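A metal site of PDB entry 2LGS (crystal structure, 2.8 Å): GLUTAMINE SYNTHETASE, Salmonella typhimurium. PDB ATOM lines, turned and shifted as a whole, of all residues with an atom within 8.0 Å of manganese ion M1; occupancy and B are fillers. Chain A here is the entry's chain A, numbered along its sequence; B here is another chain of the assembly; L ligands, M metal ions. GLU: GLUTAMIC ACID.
NH2 of Arg 339 is in salt-bridge range of OE1 of the ligand (3.6 Å). N of the ligand is in hydrogen-bond range of O of Gly 265 (2.9 Å). NH1 of Arg 359 lies within salt-bridge range of OE1 of the ligand, at 2.4 Å. N of the ligand sits at hydrogen-bond distance from OD1 of Asn 264 (2.7 Å). A nitrogen (N) of the ligand lies within salt-bridge range of the side-chain carboxylate (OE1) of Glu 131. NE2 of His 269 lies within hydrogen-bond range of OXT of the ligand, 3.4 Å away.
Of the 22 residues printed, 3 come within 4 Å of manganese ion M1. The nearest printed residue that does not touch manganese ion M1 is His 210 (4.7 Å).
Manganese ion M1 is bound by OE1 of Glu 220 (2.1 Å), OE2 of Glu 131 (2.2 Å) and OE2 of Glu 212 (2.3 Å).
The backbone carbonyl oxygen (O) of Glu 212 is in hydrogen-bond range of the backbone NH (N) of Tyr 179 (3.3 Å). O of Gln 218 is in hydrogen-bond range of N of Glu 212, 2.8 Å away. OE1 of Glu 131 is in hydrogen-bond range of N of Gly 267 (2.8 Å). The backbone carbonyl oxygen of Glu 220 sits at hydrogen-bond distance from the backbone NH of His 210, 2.9 Å away.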
ATOM      1  N   GLU A 129       0.076  -2.319  -8.113  1.00  0.00           N
ATOM      2  CA  GLU A 129      -0.343  -3.272  -9.154  1.00  0.00           C
ATOM      3  C   GLU A 129       0.793  -4.293  -9.382  1.00  0.00           C
ATOM      4  O   GLU A 129       1.502  -4.179 -10.406  1.00  0.00           O
ATOM      5  CB  GLU A 129      -0.650  -2.507 -10.476  1.00  0.00           C
ATOM      6  CG  GLU A 129      -1.575  -1.273 -10.520  1.00  0.00           C
ATOM      7  CD  GLU A 129      -1.649  -0.529 -11.890  1.00  0.00           C
ATOM      8  OE1 GLU A 129      -0.625  -0.001 -12.361  1.00  0.00           O
ATOM      9  OE2 GLU A 129      -2.748  -0.423 -12.478  1.00  0.00           O
ATOM     10  N   PRO A 130       1.089  -5.243  -8.485  1.00  0.00           N
ATOM     11  CA  PRO A 130       2.224  -6.156  -8.584  1.00  0.00           C
ATOM     12  C   PRO A 130       2.082  -7.178  -9.685  1.00  0.00           C
ATOM     13  O   PRO A 130       1.036  -7.775  -9.862  1.00  0.00           O
ATOM     14  CB  PRO A 130       2.328  -6.845  -7.256  1.00  0.00           C
ATOM     15  CG  PRO A 130       1.392  -6.088  -6.379  1.00  0.00           C
ATOM     16  CD  PRO A 130       0.302  -5.657  -7.350  1.00  0.00           C
ATOM     17  N   GLU A 131       3.115  -7.352 -10.497  1.00  0.00           N
ATOM     18  CA  GLU A 131       3.083  -8.424 -11.482  1.00  0.00           C
ATOM     19  C   GLU A 131       4.048  -9.540 -11.118  1.00  0.00           C
ATOM     20  O   GLU A 131       5.039  -9.356 -10.406  1.00  0.00           O
ATOM     21  CB  GLU A 131       3.450  -7.901 -12.822  1.00  0.00           C
ATOM     22  CG  GLU A 131       2.461  -6.868 -13.260  1.00  0.00           C
ATOM     23  CD  GLU A 131       3.001  -5.958 -14.346  1.00  0.00           C
ATOM     24  OE1 GLU A 131       4.144  -5.489 -14.304  1.00  0.00           O
ATOM     25  OE2 GLU A 131       2.237  -5.714 -15.278  1.00  0.00           O
ATOM     26  N   PHE A 132       3.759 -10.730 -11.606  1.00  0.00           N
ATOM     27  CA  PHE A 132       4.626 -11.853 -11.301  1.00  0.00           C
ATOM     28  C   PHE A 132       4.809 -12.785 -12.469  1.00  0.00           C
ATOM     29  O   PHE A 132       4.111 -12.673 -13.488  1.00  0.00           O
ATOM     30  CB  PHE A 132       4.061 -12.655 -10.111  1.00  0.00           C
ATOM     31  CG  PHE A 132       2.652 -13.203 -10.238  1.00  0.00           C
ATOM     32  CD1 PHE A 132       1.546 -12.402  -9.947  1.00  0.00           C
ATOM     33  CD2 PHE A 132       2.441 -14.530 -10.611  1.00  0.00           C
ATOM     34  CE1 PHE A 132       0.256 -12.909 -10.047  1.00  0.00           C
ATOM     35  CE2 PHE A 132       1.150 -15.037 -10.711  1.00  0.00           C
ATOM     36  CZ  PHE A 132       0.065 -14.228 -10.427  1.00  0.00           C
ATOM     37  N   TYR A 179      -0.407 -10.775 -23.643  1.00  0.00           N
ATOM     38  CA  TYR A 179      -1.529  -9.897 -23.400  1.00  0.00           C
ATOM     39  C   TYR A 179      -2.810 -10.121 -24.207  1.00  0.00           C
ATOM     40  O   TYR A 179      -3.067  -9.745 -25.347  1.00  0.00           O
ATOM     41  CB  TYR A 179      -1.102  -8.463 -23.578  1.00  0.00           C
ATOM     42  CG  TYR A 179      -1.913  -7.575 -22.659  1.00  0.00           C
ATOM     43  CD1 TYR A 179      -1.552  -7.433 -21.316  1.00  0.00           C
ATOM     44  CD2 TYR A 179      -3.020  -6.888 -23.167  1.00  0.00           C
ATOM     45  CE1 TYR A 179      -2.301  -6.591 -20.488  1.00  0.00           C
ATOM     46  CE2 TYR A 179      -3.768  -6.042 -22.360  1.00  0.00           C
ATOM     47  CZ  TYR A 179      -3.410  -5.909 -21.020  1.00  0.00           C
ATOM     48  OH  TYR A 179      -4.177  -5.083 -20.200  1.00  0.00           O
ATOM     49  N   HIS A 210      -5.615 -11.150 -14.830  1.00  0.00           N
ATOM     50  CA  HIS A 210      -5.351 -11.430 -16.224  1.00  0.00           C
ATOM     51  C   HIS A 210      -3.907 -11.775 -16.501  1.00  0.00           C
ATOM     52  O   HIS A 210      -3.009 -11.417 -15.722  1.00  0.00           O
ATOM     53  CB  HIS A 210      -5.705 -10.245 -17.085  1.00  0.00           C
ATOM     54  CG  HIS A 210      -4.902  -9.016 -16.724  1.00  0.00           C
ATOM     55  ND1 HIS A 210      -3.765  -8.616 -17.256  1.00  0.00           N
ATOM     56  CD2 HIS A 210      -5.243  -8.121 -15.748  1.00  0.00           C
ATOM     57  CE1 HIS A 210      -3.411  -7.533 -16.638  1.00  0.00           C
ATOM     58  NE2 HIS A 210      -4.298  -7.242 -15.742  1.00  0.00           N
ATOM     59  N   HIS A 211      -3.671 -12.387 -17.657  1.00  0.00           N
ATOM     60  CA  HIS A 211      -2.313 -12.649 -18.121  1.00  0.00           C
ATOM     61  C   HIS A 211      -1.639 -11.347 -18.517  1.00  0.00           C
ATOM     62  O   HIS A 211      -2.317 -10.402 -18.923  1.00  0.00           O
ATOM     63  CB  HIS A 211      -2.349 -13.556 -19.327  1.00  0.00           C
ATOM     64  CG  HIS A 211      -1.009 -14.206 -19.633  1.00  0.00           C
ATOM     65  ND1 HIS A 211       0.176 -13.655 -19.860  1.00  0.00           N
ATOM     66  CD2 HIS A 211      -0.854 -15.553 -19.770  1.00  0.00           C
ATOM     67  CE1 HIS A 211       1.030 -14.604 -20.127  1.00  0.00           C
ATOM     68  NE2 HIS A 211       0.391 -15.725 -20.057  1.00  0.00           N
ATOM     69  N   GLU A 212      -0.342 -11.197 -18.283  1.00  0.00           N
ATOM     70  CA  GLU A 212       0.356  -9.990 -18.699  1.00  0.00           C
ATOM     71  C   GLU A 212       1.085 -10.116 -20.032  1.00  0.00           C
ATOM     72  O   GLU A 212       0.963 -11.163 -20.667  1.00  0.00           O
ATOM     73  CB  GLU A 212       1.320  -9.582 -17.600  1.00  0.00           C
ATOM     74  CG  GLU A 212       0.789  -8.347 -16.872  1.00  0.00           C
ATOM     75  CD  GLU A 212       0.642  -7.057 -17.704  1.00  0.00           C
ATOM     76  OE1 GLU A 212       1.314  -6.883 -18.726  1.00  0.00           O
ATOM     77  OE2 GLU A 212      -0.142  -6.174 -17.307  1.00  0.00           O
ATOM     78  N   VAL A 213       1.860  -9.142 -20.469  1.00  0.00           N
ATOM     79  CA  VAL A 213       2.444  -9.091 -21.790  1.00  0.00           C
ATOM     80  C   VAL A 213       3.436 -10.175 -22.155  1.00  0.00           C
ATOM     81  O   VAL A 213       3.477 -10.656 -23.280  1.00  0.00           O
ATOM     82  CB  VAL A 213       3.058  -7.687 -21.928  1.00  0.00           C
ATOM     83  CG1 VAL A 213       4.151  -7.571 -22.972  1.00  0.00           C
ATOM     84  CG2 VAL A 213       1.939  -6.799 -22.433  1.00  0.00           C
ATOM     85  N   GLN A 218       3.778 -14.466 -17.547  1.00  0.00           N
ATOM     86  CA  GLN A 218       3.600 -13.250 -16.762  1.00  0.00           C
ATOM     87  C   GLN A 218       2.135 -13.088 -16.397  1.00  0.00           C
ATOM     88  O   GLN A 218       1.246 -13.255 -17.244  1.00  0.00           O
ATOM     89  CB  GLN A 218       4.038 -12.035 -17.514  1.00  0.00           C
ATOM     90  CG  GLN A 218       4.553 -11.069 -16.445  1.00  0.00           C
ATOM     91  CD  GLN A 218       4.950  -9.722 -16.995  1.00  0.00           C
ATOM     92  OE1 GLN A 218       4.530  -9.321 -18.084  1.00  0.00           O
ATOM     93  NE2 GLN A 218       5.776  -8.998 -16.235  1.00  0.00           N
ATOM     94  N   ASN A 219       1.813 -12.794 -15.143  1.00  0.00           N
ATOM     95  CA  ASN A 219       0.432 -12.675 -14.670  1.00  0.00           C
ATOM     96  C   ASN A 219       0.188 -11.524 -13.713  1.00  0.00           C
ATOM     97  O   ASN A 219       1.109 -10.915 -13.185  1.00  0.00           O
ATOM     98  CB  ASN A 219       0.047 -13.956 -14.000  1.00  0.00           C
ATOM     99  CG  ASN A 219      -0.219 -15.003 -15.051  1.00  0.00           C
ATOM    100  OD1 ASN A 219       0.580 -15.886 -15.328  1.00  0.00           O
ATOM    101  ND2 ASN A 219      -1.297 -14.998 -15.775  1.00  0.00           N
ATOM    102  N   GLU A 220      -1.083 -11.174 -13.539  1.00  0.00           N
ATOM    103  CA  GLU A 220      -1.469 -10.081 -12.650  1.00  0.00           C
ATOM    104  C   GLU A 220      -2.821 -10.302 -12.003  1.00  0.00           C
ATOM    105  O   GLU A 220      -3.814 -10.579 -12.676  1.00  0.00           O
ATOM    106  CB  GLU A 220      -1.499  -8.809 -13.427  1.00  0.00           C
ATOM    107  CG  GLU A 220      -1.502  -7.553 -12.572  1.00  0.00           C
ATOM    108  CD  GLU A 220      -1.471  -6.287 -13.426  1.00  0.00           C
ATOM    109  OE1 GLU A 220      -0.931  -6.350 -14.522  1.00  0.00           O
ATOM    110  OE2 GLU A 220      -1.986  -5.245 -13.023  1.00  0.00           O
ATOM    111  N   VAL A 221      -2.807 -10.234 -10.682  1.00  0.00           N
ATOM    112  CA  VAL A 221      -4.049 -10.230  -9.933  1.00  0.00           C
ATOM    113  C   VAL A 221      -4.184  -8.826  -9.370  1.00  0.00           C
ATOM    114  O   VAL A 221      -3.351  -8.370  -8.586  1.00  0.00           O
ATOM    115  CB  VAL A 221      -4.002 -11.267  -8.820  1.00  0.00           C
ATOM    116  CG1 VAL A 221      -5.292 -11.237  -8.039  1.00  0.00           C
ATOM    117  CG2 VAL A 221      -3.877 -12.653  -9.406  1.00  0.00           C
ATOM    118  N   ASN A 264       8.892  -8.386 -21.499  1.00  0.00           N
ATOM    119  CA  ASN A 264       8.458  -7.636 -20.342  1.00  0.00           C
ATOM    120  C   ASN A 264       9.008  -8.007 -18.958  1.00  0.00           C
ATOM    121  O   ASN A 264       9.311  -9.157 -18.627  1.00  0.00           O
ATOM    122  CB  ASN A 264       6.947  -7.699 -20.330  1.00  0.00           C
ATOM    123  CG  ASN A 264       6.292  -6.400 -19.902  1.00  0.00           C
ATOM    124  OD1 ASN A 264       5.424  -6.329 -19.030  1.00  0.00           O
ATOM    125  ND2 ASN A 264       6.656  -5.302 -20.531  1.00  0.00           N
ATOM    126  N   GLY A 265       9.101  -6.959 -18.160  1.00  0.00           N
ATOM    127  CA  GLY A 265       9.488  -7.095 -16.771  1.00  0.00           C
ATOM    128  C   GLY A 265       8.254  -6.945 -15.884  1.00  0.00           C
ATOM    129  O   GLY A 265       7.161  -6.511 -16.263  1.00  0.00           O
ATOM    130  N   SER A 266       8.396  -7.387 -14.666  1.00  0.00           N
ATOM    131  CA  SER A 266       7.336  -7.263 -13.697  1.00  0.00           C
ATOM    132  C   SER A 266       7.525  -5.986 -12.891  1.00  0.00           C
ATOM    133  O   SER A 266       8.491  -5.794 -12.142  1.00  0.00           O
ATOM    134  CB  SER A 266       7.350  -8.477 -12.789  1.00  0.00           C
ATOM    135  OG  SER A 266       6.964  -9.632 -13.520  1.00  0.00           O
ATOM    136  N   GLY A 267       6.627  -5.038 -13.089  1.00  0.00           N
ATOM    137  CA  GLY A 267       6.601  -3.843 -12.266  1.00  0.00           C
ATOM    138  C   GLY A 267       5.461  -3.814 -11.256  1.00  0.00           C
ATOM    139  O   GLY A 267       4.446  -4.522 -11.391  1.00  0.00           O
ATOM    140  N   MET A 268       5.563  -3.013 -10.208  1.00  0.00           N
ATOM    141  CA  MET A 268       4.502  -2.850  -9.226  1.00  0.00           C
ATOM    142  C   MET A 268       4.151  -1.367  -9.171  1.00  0.00           C
ATOM    143  O   MET A 268       4.697  -0.593  -8.399  1.00  0.00           O
ATOM    144  CB  MET A 268       4.969  -3.287  -7.837  1.00  0.00           C
ATOM    145  CG  MET A 268       3.916  -3.244  -6.748  1.00  0.00           C
ATOM    146  SD  MET A 268       4.767  -3.057  -5.160  1.00  0.00           S
ATOM    147  CE  MET A 268       4.627  -4.699  -4.528  1.00  0.00           C
ATOM    148  N   HIS A 269       3.213  -0.929 -10.002  1.00  0.00           N
ATOM    149  CA  HIS A 269       2.870   0.492 -10.006  1.00  0.00           C
ATOM    150  C   HIS A 269       2.061   0.885  -8.801  1.00  0.00           C
ATOM    151  O   HIS A 269       1.030   0.277  -8.526  1.00  0.00           O
ATOM    152  CB  HIS A 269       2.018   0.952 -11.159  1.00  0.00           C
ATOM    153  CG  HIS A 269       2.482   0.586 -12.562  1.00  0.00           C
ATOM    154  ND1 HIS A 269       2.051   1.128 -13.703  1.00  0.00           N
ATOM    155  CD2 HIS A 269       3.466  -0.336 -12.846  1.00  0.00           C
ATOM    156  CE1 HIS A 269       2.778   0.545 -14.631  1.00  0.00           C
ATOM    157  NE2 HIS A 269       3.602  -0.307 -14.136  1.00  0.00           N
ATOM    158  N   ARG A 339       2.492   7.570 -21.801  1.00  0.00           N
ATOM    159  CA  ARG A 339       2.946   6.354 -21.090  1.00  0.00           C
ATOM    160  C   ARG A 339       4.370   6.082 -21.623  1.00  0.00           C
ATOM    161  O   ARG A 339       4.661   5.460 -22.646  1.00  0.00           O
ATOM    162  CB  ARG A 339       2.076   5.086 -21.352  1.00  0.00           C
ATOM    163  CG  ARG A 339       0.569   5.102 -21.039  1.00  0.00           C
ATOM    164  CD  ARG A 339      -0.015   4.196 -19.931  1.00  0.00           C
ATOM    165  NE  ARG A 339      -0.027   2.738 -20.107  1.00  0.00           N
ATOM    166  CZ  ARG A 339      -1.021   1.952 -19.632  1.00  0.00           C
ATOM    167  NH1 ARG A 339      -2.150   2.424 -19.115  1.00  0.00           N
ATOM    168  NH2 ARG A 339      -0.882   0.629 -19.673  1.00  0.00           N
ATOM    169  N   ARG A 359       4.484   4.789 -11.969  1.00  0.00           N
ATOM    170  CA  ARG A 359       4.756   3.560 -12.699  1.00  0.00           C
ATOM    171  C   ARG A 359       6.079   2.856 -12.472  1.00  0.00           C
ATOM    172  O   ARG A 359       6.180   1.674 -12.772  1.00  0.00           O
ATOM    173  CB  ARG A 359       4.669   3.798 -14.184  1.00  0.00           C
ATOM    174  CG  ARG A 359       3.298   4.179 -14.657  1.00  0.00           C
ATOM    175  CD  ARG A 359       3.336   3.945 -16.126  1.00  0.00           C
ATOM    176  NE  ARG A 359       2.105   3.314 -16.572  1.00  0.00           N
ATOM    177  CZ  ARG A 359       2.082   2.156 -17.233  1.00  0.00           C
ATOM    178  NH1 ARG A 359       3.131   1.342 -17.409  1.00  0.00           N
ATOM    179  NH2 ARG A 359       0.933   1.713 -17.667  1.00  0.00           N
ATOM    180  N   ASP B  50      -6.095  -1.036 -20.565  1.00  0.00           N
ATOM    181  CA  ASP B  50      -5.121  -0.495 -21.469  1.00  0.00           C
ATOM    182  C   ASP B  50      -5.149  -1.187 -22.839  1.00  0.00           C
ATOM    183  O   ASP B  50      -4.571  -2.241 -23.115  1.00  0.00           O
ATOM    184  CB  ASP B  50      -3.733  -0.600 -20.890  1.00  0.00           C
ATOM    185  CG  ASP B  50      -2.727   0.068 -21.826  1.00  0.00           C
ATOM    186  OD1 ASP B  50      -2.874   1.271 -22.086  1.00  0.00           O
ATOM    187  OD2 ASP B  50      -1.804  -0.614 -22.280  1.00  0.00           O
HETATM  188  N   GLU L   1       4.874  -4.835 -16.822  1.00  0.00           N
HETATM  189  CA  GLU L   1       5.207  -3.432 -17.001  1.00  0.00           C
HETATM  190  C   GLU L   1       6.384  -2.955 -16.141  1.00  0.00           C
HETATM  191  O   GLU L   1       7.493  -3.497 -16.371  1.00  0.00           O
HETATM  192  CB  GLU L   1       3.975  -2.622 -16.671  1.00  0.00           C
HETATM  193  CG  GLU L   1       2.868  -2.936 -17.671  1.00  0.00           C
HETATM  194  CD  GLU L   1       1.705  -1.954 -17.755  1.00  0.00           C
HETATM  195  OE1 GLU L   1       1.921  -0.736 -17.835  1.00  0.00           O
HETATM  196  OE2 GLU L   1       0.585  -2.462 -17.786  1.00  0.00           O
HETATM  197  OXT GLU L   1       6.240  -2.049 -15.312  1.00  0.00           O
HETATM  198 MN    MN M   1       0.205  -4.821 -15.454  1.00  0.00          MN
HETATM  199 MN    MN M   2      -0.994   0.966 -14.337  1.00  0.00          MN
